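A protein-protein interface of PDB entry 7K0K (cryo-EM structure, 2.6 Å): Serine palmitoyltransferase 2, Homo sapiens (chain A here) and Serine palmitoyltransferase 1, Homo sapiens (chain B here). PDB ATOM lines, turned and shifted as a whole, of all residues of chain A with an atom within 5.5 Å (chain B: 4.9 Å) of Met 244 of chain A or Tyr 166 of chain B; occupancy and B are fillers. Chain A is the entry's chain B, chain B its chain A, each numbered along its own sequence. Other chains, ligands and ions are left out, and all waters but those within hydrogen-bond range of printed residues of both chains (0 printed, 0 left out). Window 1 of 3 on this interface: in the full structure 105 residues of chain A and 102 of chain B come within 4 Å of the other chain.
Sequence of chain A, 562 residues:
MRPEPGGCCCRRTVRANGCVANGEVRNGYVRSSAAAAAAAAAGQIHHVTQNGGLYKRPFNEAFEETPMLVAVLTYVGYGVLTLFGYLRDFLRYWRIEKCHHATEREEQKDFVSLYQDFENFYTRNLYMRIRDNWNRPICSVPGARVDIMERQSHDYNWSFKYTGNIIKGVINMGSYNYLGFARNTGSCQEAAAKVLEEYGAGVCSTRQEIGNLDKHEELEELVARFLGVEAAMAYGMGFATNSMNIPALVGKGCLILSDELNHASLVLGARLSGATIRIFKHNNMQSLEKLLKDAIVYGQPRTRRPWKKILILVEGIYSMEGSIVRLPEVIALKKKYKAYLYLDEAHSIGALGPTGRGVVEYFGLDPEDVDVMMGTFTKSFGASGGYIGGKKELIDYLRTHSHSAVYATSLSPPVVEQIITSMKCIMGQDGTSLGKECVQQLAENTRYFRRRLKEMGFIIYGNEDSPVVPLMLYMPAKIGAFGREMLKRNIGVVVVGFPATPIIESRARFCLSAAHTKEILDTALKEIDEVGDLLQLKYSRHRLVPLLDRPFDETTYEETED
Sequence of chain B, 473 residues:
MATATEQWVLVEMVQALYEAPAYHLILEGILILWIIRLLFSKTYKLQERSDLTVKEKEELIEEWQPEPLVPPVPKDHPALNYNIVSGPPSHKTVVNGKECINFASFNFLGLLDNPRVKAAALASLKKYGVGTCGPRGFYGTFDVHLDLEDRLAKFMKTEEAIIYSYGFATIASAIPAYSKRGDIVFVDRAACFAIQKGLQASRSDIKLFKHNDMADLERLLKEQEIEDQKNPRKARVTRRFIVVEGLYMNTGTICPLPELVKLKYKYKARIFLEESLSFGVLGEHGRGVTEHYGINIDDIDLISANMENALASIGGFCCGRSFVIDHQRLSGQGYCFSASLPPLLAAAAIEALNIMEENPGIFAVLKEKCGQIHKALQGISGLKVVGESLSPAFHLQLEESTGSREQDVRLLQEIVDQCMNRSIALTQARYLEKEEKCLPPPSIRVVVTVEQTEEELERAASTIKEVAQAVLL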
ATOM      1  N   TYR A 235      17.625 -25.887 -16.830  1.00  0.00           N
ATOM      2  CA  TYR A 235      18.531 -25.517 -17.903  1.00  0.00           C
ATOM      3  C   TYR A 235      18.721 -24.008 -17.902  1.00  0.00           C
ATOM      4  O   TYR A 235      17.899 -23.259 -17.371  1.00  0.00           O
ATOM      5  CB  TYR A 235      18.011 -25.981 -19.268  1.00  0.00           C
ATOM      6  CG  TYR A 235      17.586 -27.426 -19.285  1.00  0.00           C
ATOM      7  CD1 TYR A 235      18.519 -28.436 -19.433  1.00  0.00           C
ATOM      8  CD2 TYR A 235      16.257 -27.779 -19.146  1.00  0.00           C
ATOM      9  CE1 TYR A 235      18.143 -29.752 -19.442  1.00  0.00           C
ATOM     10  CE2 TYR A 235      15.870 -29.095 -19.153  1.00  0.00           C
ATOM     11  CZ  TYR A 235      16.817 -30.077 -19.303  1.00  0.00           C
ATOM     12  OH  TYR A 235      16.439 -31.396 -19.312  1.00  0.00           O
ATOM     13  N   GLY A 236      19.817 -23.572 -18.520  1.00  0.00           N
ATOM     14  CA  GLY A 236      20.178 -22.165 -18.459  1.00  0.00           C
ATOM     15  C   GLY A 236      19.281 -21.270 -19.291  1.00  0.00           C
ATOM     16  O   GLY A 236      19.194 -20.068 -19.043  1.00  0.00           O
ATOM     17  N   MET A 237      18.612 -21.836 -20.292  1.00  0.00           N
ATOM     18  CA  MET A 237      17.764 -21.061 -21.186  1.00  0.00           C
ATOM     19  C   MET A 237      16.566 -21.893 -21.618  1.00  0.00           C
ATOM     20  O   MET A 237      16.691 -23.098 -21.844  1.00  0.00           O
ATOM     21  CB  MET A 237      18.572 -20.581 -22.399  1.00  0.00           C
ATOM     22  CG  MET A 237      17.776 -19.899 -23.482  1.00  0.00           C
ATOM     23  SD  MET A 237      18.838 -19.152 -24.726  1.00  0.00           S
ATOM     24  CE  MET A 237      18.879 -20.433 -25.961  1.00  0.00           C
ATOM     25  N   PHE A 239      14.596 -21.399 -24.440  1.00  0.00           N
ATOM     26  CA  PHE A 239      14.812 -21.723 -25.845  1.00  0.00           C
ATOM     27  C   PHE A 239      15.723 -22.933 -25.975  1.00  0.00           C
ATOM     28  O   PHE A 239      15.445 -23.854 -26.754  1.00  0.00           O
ATOM     29  CB  PHE A 239      15.408 -20.510 -26.556  1.00  0.00           C
ATOM     30  CG  PHE A 239      15.436 -20.621 -28.049  1.00  0.00           C
ATOM     31  CD1 PHE A 239      16.431 -21.335 -28.687  1.00  0.00           C
ATOM     32  CD2 PHE A 239      14.491 -19.975 -28.815  1.00  0.00           C
ATOM     33  CE1 PHE A 239      16.459 -21.428 -30.053  1.00  0.00           C
ATOM     34  CE2 PHE A 239      14.515 -20.066 -30.182  1.00  0.00           C
ATOM     35  CZ  PHE A 239      15.500 -20.793 -30.802  1.00  0.00           C
ATOM     36  N   ALA A 240      16.805 -22.951 -25.200  1.00  0.00           N
ATOM     37  CA  ALA A 240      17.685 -24.107 -25.163  1.00  0.00           C
ATOM     38  C   ALA A 240      16.979 -25.330 -24.610  1.00  0.00           C
ATOM     39  O   ALA A 240      17.203 -26.434 -25.102  1.00  0.00           O
ATOM     40  CB  ALA A 240      18.925 -23.797 -24.331  1.00  0.00           C
ATOM     41  N   THR A 241      16.132 -25.162 -23.594  1.00  0.00           N
ATOM     42  CA  THR A 241      15.398 -26.302 -23.056  1.00  0.00           C
ATOM     43  C   THR A 241      14.664 -27.036 -24.166  1.00  0.00           C
ATOM     44  O   THR A 241      14.861 -28.241 -24.371  1.00  0.00           O
ATOM     45  CB  THR A 241      14.413 -25.836 -21.986  1.00  0.00           C
ATOM     46  OG1 THR A 241      15.122 -25.181 -20.931  1.00  0.00           O
ATOM     47  CG2 THR A 241      13.652 -27.006 -21.421  1.00  0.00           C
ATOM     48  N   ASN A 242      13.872 -26.300 -24.943  1.00  0.00           N
ATOM     49  CA  ASN A 242      13.173 -26.909 -26.071  1.00  0.00           C
ATOM     50  C   ASN A 242      14.149 -27.489 -27.085  1.00  0.00           C
ATOM     51  O   ASN A 242      14.150 -28.702 -27.343  1.00  0.00           O
ATOM     52  CB  ASN A 242      12.272 -25.877 -26.733  1.00  0.00           C
ATOM     53  CG  ASN A 242      10.877 -25.902 -26.192  1.00  0.00           C
ATOM     54  OD1 ASN A 242      10.401 -26.936 -25.737  1.00  0.00           O
ATOM     55  ND2 ASN A 242      10.213 -24.758 -26.211  1.00  0.00           N
ATOM     56  N   SER A 243      15.005 -26.634 -27.657  1.00  0.00           N
ATOM     57  CA  SER A 243      15.810 -27.023 -28.809  1.00  0.00           C
ATOM     58  C   SER A 243      16.788 -28.138 -28.474  1.00  0.00           C
ATOM     59  O   SER A 243      17.328 -28.786 -29.377  1.00  0.00           O
ATOM     60  CB  SER A 243      16.565 -25.813 -29.348  1.00  0.00           C
ATOM     61  OG  SER A 243      15.678 -24.758 -29.654  1.00  0.00           O
ATOM     62  N   MET A 244      17.036 -28.379 -27.192  1.00  0.00           N
ATOM     63  CA  MET A 244      18.048 -29.328 -26.775  1.00  0.00           C
ATOM     64  C   MET A 244      17.458 -30.567 -26.131  1.00  0.00           C
ATOM     65  O   MET A 244      18.169 -31.559 -25.973  1.00  0.00           O
ATOM     66  CB  MET A 244      18.997 -28.655 -25.793  1.00  0.00           C
ATOM     67  CG  MET A 244      19.820 -27.565 -26.417  1.00  0.00           C
ATOM     68  SD  MET A 244      20.890 -26.825 -25.192  1.00  0.00           S
ATOM     69  CE  MET A 244      21.619 -25.545 -26.170  1.00  0.00           C
ATOM     70  N   ASN A 245      16.187 -30.541 -25.742  1.00  0.00           N
ATOM     71  CA  ASN A 245      15.601 -31.718 -25.132  1.00  0.00           C
ATOM     72  C   ASN A 245      14.537 -32.385 -25.978  1.00  0.00           C
ATOM     73  O   ASN A 245      14.267 -33.566 -25.770  1.00  0.00           O
ATOM     74  CB  ASN A 245      15.009 -31.358 -23.773  1.00  0.00           C
ATOM     75  CG  ASN A 245      16.035 -30.768 -22.845  1.00  0.00           C
ATOM     76  OD1 ASN A 245      17.142 -31.278 -22.724  1.00  0.00           O
ATOM     77  ND2 ASN A 245      15.690 -29.660 -22.217  1.00  0.00           N
ATOM     78  N   ILE A 246      13.911 -31.673 -26.919  1.00  0.00           N
ATOM     79  CA  ILE A 246      13.051 -32.349 -27.893  1.00  0.00           C
ATOM     80  C   ILE A 246      13.842 -33.330 -28.745  1.00  0.00           C
ATOM     81  O   ILE A 246      13.356 -34.448 -28.970  1.00  0.00           O
ATOM     82  CB  ILE A 246      12.265 -31.319 -28.714  1.00  0.00           C
ATOM     83  CG1 ILE A 246      11.340 -30.520 -27.805  1.00  0.00           C
ATOM     84  CG2 ILE A 246      11.445 -32.012 -29.774  1.00  0.00           C
ATOM     85  CD1 ILE A 246      10.608 -29.420 -28.515  1.00  0.00           C
ATOM     86  N   PRO A 247      15.041 -33.008 -29.251  1.00  0.00           N
ATOM     87  CA  PRO A 247      15.789 -34.011 -30.024  1.00  0.00           C
ATOM     88  C   PRO A 247      16.148 -35.257 -29.241  1.00  0.00           C
ATOM     89  O   PRO A 247      16.381 -36.309 -29.847  1.00  0.00           O
ATOM     90  CB  PRO A 247      17.044 -33.243 -30.452  1.00  0.00           C
ATOM     91  CG  PRO A 247      16.618 -31.849 -30.484  1.00  0.00           C
ATOM     92  CD  PRO A 247      15.696 -31.692 -29.330  1.00  0.00           C
ATOM     93  N   ALA A 248      16.222 -35.173 -27.915  1.00  0.00           N
ATOM     94  CA  ALA A 248      16.554 -36.349 -27.120  1.00  0.00           C
ATOM     95  C   ALA A 248      15.365 -37.296 -27.016  1.00  0.00           C
ATOM     96  O   ALA A 248      15.536 -38.519 -26.981  1.00  0.00           O
ATOM     97  CB  ALA A 248      17.029 -35.925 -25.733  1.00  0.00           C
ATOM     98  N   GLY A 269      13.369 -27.405 -32.049  1.00  0.00           N
ATOM     99  CA  GLY A 269      13.568 -28.695 -31.415  1.00  0.00           C
ATOM    100  C   GLY A 269      13.002 -29.833 -32.237  1.00  0.00           C
ATOM    101  O   GLY A 269      13.597 -30.908 -32.318  1.00  0.00           O
ATOM    102  N   HIS A 401      21.183 -37.737 -21.378  1.00  0.00           N
ATOM    103  CA  HIS A 401      21.181 -37.620 -22.831  1.00  0.00           C
ATOM    104  C   HIS A 401      20.774 -36.247 -23.352  1.00  0.00           C
ATOM    105  O   HIS A 401      20.677 -36.072 -24.569  1.00  0.00           O
ATOM    106  CB  HIS A 401      20.256 -38.672 -23.443  1.00  0.00           C
ATOM    107  CG  HIS A 401      20.766 -40.072 -23.330  1.00  0.00           C
ATOM    108  ND1 HIS A 401      20.492 -40.880 -22.250  1.00  0.00           N
ATOM    109  CD2 HIS A 401      21.523 -40.813 -24.171  1.00  0.00           C
ATOM    110  CE1 HIS A 401      21.064 -42.057 -22.426  1.00  0.00           C
ATOM    111  NE2 HIS A 401      21.697 -42.042 -23.585  1.00  0.00           N
ATOM    112  N   SER A 402      20.516 -35.278 -22.485  1.00  0.00           N
ATOM    113  CA  SER A 402      20.168 -33.950 -22.972  1.00  0.00           C
ATOM    114  C   SER A 402      21.399 -33.268 -23.549  1.00  0.00           C
ATOM    115  O   SER A 402      22.510 -33.427 -23.040  1.00  0.00           O
ATOM    116  CB  SER A 402      19.577 -33.101 -21.851  1.00  0.00           C
ATOM    117  OG  SER A 402      19.654 -31.724 -22.154  1.00  0.00           O
ATOM    118  N   HIS A 403      21.203 -32.512 -24.629  1.00  0.00           N
ATOM    119  CA  HIS A 403      22.325 -31.793 -25.223  1.00  0.00           C
ATOM    120  C   HIS A 403      22.851 -30.736 -24.263  1.00  0.00           C
ATOM    121  O   HIS A 403      24.061 -30.493 -24.193  1.00  0.00           O
ATOM    122  CB  HIS A 403      21.907 -31.148 -26.542  1.00  0.00           C
ATOM    123  CG  HIS A 403      21.361 -32.113 -27.548  1.00  0.00           C
ATOM    124  ND1 HIS A 403      22.144 -33.044 -28.190  1.00  0.00           N
ATOM    125  CD2 HIS A 403      20.116 -32.260 -28.055  1.00  0.00           C
ATOM    126  CE1 HIS A 403      21.399 -33.744 -29.026  1.00  0.00           C
ATOM    127  NE2 HIS A 403      20.164 -33.285 -28.965  1.00  0.00           N
ATOM    128  N   SER A 404      21.946 -30.094 -23.523  1.00  0.00           N
ATOM    129  CA  SER A 404      22.338 -29.060 -22.575  1.00  0.00           C
ATOM    130  C   SER A 404      23.111 -29.647 -21.404  1.00  0.00           C
ATOM    131  O   SER A 404      24.009 -29.000 -20.855  1.00  0.00           O
ATOM    132  CB  SER A 404      21.101 -28.319 -22.078  1.00  0.00           C
ATOM    133  OG  SER A 404      21.453 -27.287 -21.178  1.00  0.00           O
ATOM    134  N   ALA A 408      26.407 -27.688 -22.579  1.00  0.00           N
ATOM    135  CA  ALA A 408      26.059 -26.313 -22.265  1.00  0.00           C
ATOM    136  C   ALA A 408      26.321 -26.010 -20.798  1.00  0.00           C
ATOM    137  O   ALA A 408      26.174 -26.874 -19.930  1.00  0.00           O
ATOM    138  CB  ALA A 408      24.602 -26.031 -22.603  1.00  0.00           C
ATOM    139  N   THR A 409      26.707 -24.767 -20.534  1.00  0.00           N
ATOM    140  CA  THR A 409      27.023 -24.333 -19.182  1.00  0.00           C
ATOM    141  C   THR A 409      25.764 -24.287 -18.321  1.00  0.00           C
ATOM    142  O   THR A 409      24.672 -23.963 -18.791  1.00  0.00           O
ATOM    143  CB  THR A 409      27.693 -22.960 -19.219  1.00  0.00           C
ATOM    144  OG1 THR A 409      28.865 -23.030 -20.038  1.00  0.00           O
ATOM    145  CG2 THR A 409      28.097 -22.516 -17.835  1.00  0.00           C
ATOM    146  N   TYR B 164      24.366 -13.010 -26.984  1.00  0.00           N
ATOM    147  CA  TYR B 164      23.396 -14.065 -26.752  1.00  0.00           C
ATOM    148  C   TYR B 164      23.402 -14.427 -25.275  1.00  0.00           C
ATOM    149  O   TYR B 164      24.423 -14.300 -24.595  1.00  0.00           O
ATOM    150  CB  TYR B 164      23.714 -15.310 -27.577  1.00  0.00           C
ATOM    151  CG  TYR B 164      23.428 -15.186 -29.050  1.00  0.00           C
ATOM    152  CD1 TYR B 164      24.286 -14.494 -29.885  1.00  0.00           C
ATOM    153  CD2 TYR B 164      22.315 -15.785 -29.609  1.00  0.00           C
ATOM    154  CE1 TYR B 164      24.038 -14.390 -31.227  1.00  0.00           C
ATOM    155  CE2 TYR B 164      22.060 -15.686 -30.952  1.00  0.00           C
ATOM    156  CZ  TYR B 164      22.923 -14.986 -31.755  1.00  0.00           C
ATOM    157  OH  TYR B 164      22.668 -14.884 -33.099  1.00  0.00           O
ATOM    158  N   SER B 165      22.256 -14.896 -24.788  1.00  0.00           N
ATOM    159  CA  SER B 165      22.126 -15.179 -23.364  1.00  0.00           C
ATOM    160  C   SER B 165      22.568 -16.599 -23.027  1.00  0.00           C
ATOM    161  O   SER B 165      22.493 -17.013 -21.867  1.00  0.00           O
ATOM    162  CB  SER B 165      20.687 -14.940 -22.919  1.00  0.00           C
ATOM    163  OG  SER B 165      19.785 -15.743 -23.655  1.00  0.00           O
ATOM    164  N   TYR B 166      23.030 -17.358 -24.017  1.00  0.00           N
ATOM    165  CA  TYR B 166      23.415 -18.746 -23.813  1.00  0.00           C
ATOM    166  C   TYR B 166      24.591 -19.089 -24.714  1.00  0.00           C
ATOM    167  O   TYR B 166      24.594 -18.744 -25.898  1.00  0.00           O
ATOM    168  CB  TYR B 166      22.231 -19.660 -24.094  1.00  0.00           C
ATOM    169  CG  TYR B 166      22.252 -20.984 -23.379  1.00  0.00           C
ATOM    170  CD1 TYR B 166      22.133 -21.039 -22.004  1.00  0.00           C
ATOM    171  CD2 TYR B 166      22.304 -22.177 -24.077  1.00  0.00           C
ATOM    172  CE1 TYR B 166      22.124 -22.230 -21.341  1.00  0.00           C
ATOM    173  CE2 TYR B 166      22.291 -23.382 -23.417  1.00  0.00           C
ATOM    174  CZ  TYR B 166      22.198 -23.399 -22.047  1.00  0.00           C
ATOM    175  OH  TYR B 166      22.177 -24.587 -21.362  1.00  0.00           O
ATOM    176  N   GLY B 167      25.589 -19.770 -24.149  1.00  0.00           N
ATOM    177  CA  GLY B 167      26.827 -20.008 -24.873  1.00  0.00           C
ATOM    178  C   GLY B 167      26.692 -20.951 -26.051  1.00  0.00           C
ATOM    179  O   GLY B 167      27.345 -20.763 -27.077  1.00  0.00           O
ATOM    180  N   PHE B 168      25.886 -22.001 -25.908  1.00  0.00           N
ATOM    181  CA  PHE B 168      25.626 -22.910 -27.022  1.00  0.00           C
ATOM    182  C   PHE B 168      24.884 -22.188 -28.141  1.00  0.00           C
ATOM    183  O   PHE B 168      25.225 -22.315 -29.331  1.00  0.00           O
ATOM    184  CB  PHE B 168      24.805 -24.085 -26.495  1.00  0.00           C
ATOM    185  CG  PHE B 168      24.826 -25.311 -27.359  1.00  0.00           C
ATOM    186  CD1 PHE B 168      23.970 -25.440 -28.438  1.00  0.00           C
ATOM    187  CD2 PHE B 168      25.691 -26.347 -27.074  1.00  0.00           C
ATOM    188  CE1 PHE B 168      23.978 -26.577 -29.208  1.00  0.00           C
ATOM    189  CE2 PHE B 168      25.702 -27.484 -27.843  1.00  0.00           C
ATOM    190  CZ  PHE B 168      24.843 -27.600 -28.911  1.00  0.00           C
ATOM    191  N   ALA B 169      23.888 -21.387 -27.761  1.00  0.00           N
ATOM    192  CA  ALA B 169      22.973 -20.795 -28.722  1.00  0.00           C
ATOM    193  C   ALA B 169      23.654 -19.778 -29.618  1.00  0.00           C
ATOM    194  O   ALA B 169      23.218 -19.589 -30.753  1.00  0.00           O
ATOM    195  CB  ALA B 169      21.802 -20.143 -27.997  1.00  0.00           C
ATOM    196  N   THR B 170      24.720 -19.124 -29.151  1.00  0.00           N
ATOM    197  CA  THR B 170      25.311 -18.065 -29.963  1.00  0.00           C
ATOM    198  C   THR B 170      25.767 -18.597 -31.315  1.00  0.00           C
ATOM    199  O   THR B 170      25.334 -18.096 -32.356  1.00  0.00           O
ATOM    200  CB  THR B 170      26.453 -17.366 -29.218  1.00  0.00           C
ATOM    201  OG1 THR B 170      27.012 -16.350 -30.057  1.00  0.00           O
ATOM    202  CG2 THR B 170      27.544 -18.315 -28.810  1.00  0.00           C
ATOM    203  N   GLU B 308      31.572 -17.622 -21.136  1.00  0.00           N
ATOM    204  CA  GLU B 308      31.474 -18.513 -19.989  1.00  0.00           C
ATOM    205  C   GLU B 308      32.808 -19.094 -19.548  1.00  0.00           C
ATOM    206  O   GLU B 308      32.899 -19.583 -18.419  1.00  0.00           O
ATOM    207  CB  GLU B 308      30.504 -19.649 -20.312  1.00  0.00           C
ATOM    208  CG  GLU B 308      29.053 -19.211 -20.340  1.00  0.00           C
ATOM    209  CD  GLU B 308      28.204 -20.045 -21.266  1.00  0.00           C
ATOM    210  OE1 GLU B 308      28.770 -20.691 -22.169  1.00  0.00           O
ATOM    211  OE2 GLU B 308      26.968 -20.049 -21.098  1.00  0.00           O
ATOM    212  N   GLY B 315      26.631 -16.612 -21.017  1.00  0.00           N
ATOM    213  CA  GLY B 315      26.356 -15.899 -22.248  1.00  0.00           C
ATOM    214  C   GLY B 315      27.332 -16.162 -23.375  1.00  0.00           C
ATOM    215  O   GLY B 315      28.342 -16.839 -23.188  1.00  0.00           O
ATOM    216  N   GLY B 316      27.033 -15.629 -24.555  1.00  0.00           N
ATOM    217  CA  GLY B 316      27.942 -15.718 -25.676  1.00  0.00           C
ATOM    218  C   GLY B 316      27.888 -14.436 -26.478  1.00  0.00           C
ATOM    219  O   GLY B 316      27.055 -13.569 -26.232  1.00  0.00           O
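OH of Tyr 166 of chain B is in hydrogen-bond range of OG of Ser 404 of chain A.
OG of Ser 165 of chain B sits at hydrogen-bond distance from SD of Met 237 of chain A, 3.7 Å away.
The side-chain carboxylate (OE1) of Glu 308 of chain B is in hydrogen-bond range of the side-chain hydroxyl (OG1) of Thr 409 of chain A, 3.2 Å away.
N of Gly 167 of chain B sits at hydrogen-bond distance from OE2 of Glu 308 of chain B, 3.4 Å away.
The side-chain hydroxyl (OG) of Ser 402 of chain A lies within hydrogen-bond range of the backbone NH (N) of Ser 404 of chain A, at 3.1 Å.
O of Met 237 of chain A sits at hydrogen-bond distance from OG1 of Thr 241 of chain A (2.8 Å).
The side-chain carboxylate (OE2) of Glu 308 of chain B sits at hydrogen-bond distance from the backbone NH (N) of Gly 315 of chain B (3.5 Å).
O of Met 244 of chain A lies close to N of His 403 of chain A, at 3.5 Å.
Gly 236 of chain A touches Tyr 166 of chain B (CA to CE1, 3.5 Å).
CB of Tyr 166 of chain B touches SD of Met 237 of chain A (3.5 Å).
CB of Ala 169 of chain B touches CE of Met 237 of chain A, at 3.6 Å.
Ala 240 of chain A touches Tyr 166 of chain B (CB to CE2, 3.5 Å).
CE of Met 244 of chain A touches CE2 of Tyr 166 of chain B (3.6 Å).
Met 244 of chain A touches Phe 168 of chain B.
OH of Tyr 166 of chain B touches CB of Ala 408 of chain A, 3.1 Å away.
Tyr 166 of chain B touches Thr 409 of chain A.
Met 244 of chain A touches just these residues of chain B: Tyr 166 (3.6 Å) and Phe 168 (3.3 Å).
Gly 269 of chain A touches none of the printed residues of chain B.
Of the printed residues of chain B, Ser 404 of chain A touches Tyr 166.
Tyr 164 of chain B touches none of the printed residues of chain A.
Tyr 166 of chain B touches seven residues of chain A.
Printed residues of chain A within 4 Å of Ala 169 of chain B: Met 237.
The nearest printed residue of chain B that does not touch Met 244 of chain A is Ala 169 of chain B (5.0 Å).
The nearest printed residue of chain B that does not touch Gly 236 of chain A is Ser 165 of chain B (5.3 Å).
Of the 10 printed residues of chain B, 5 touch a printed residue of chain A.
Printed residues of chain B that touch a printed residue of chain A: Ser 165, Tyr 166, Phe 168, Ala 169 and Glu 308.
Hydrophobic or aromatic side chains of chain B that line the printed part of chain A: Tyr 166, Phe 168 and Ala 169.
Printed residues of chain A that touch a printed residue of chain B: Gly 236, Met 237, Ala 240, Met 244, Ser 404, Ala 408 and Thr 409.
Among the printed residues, 11 pairs touch across the chains.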
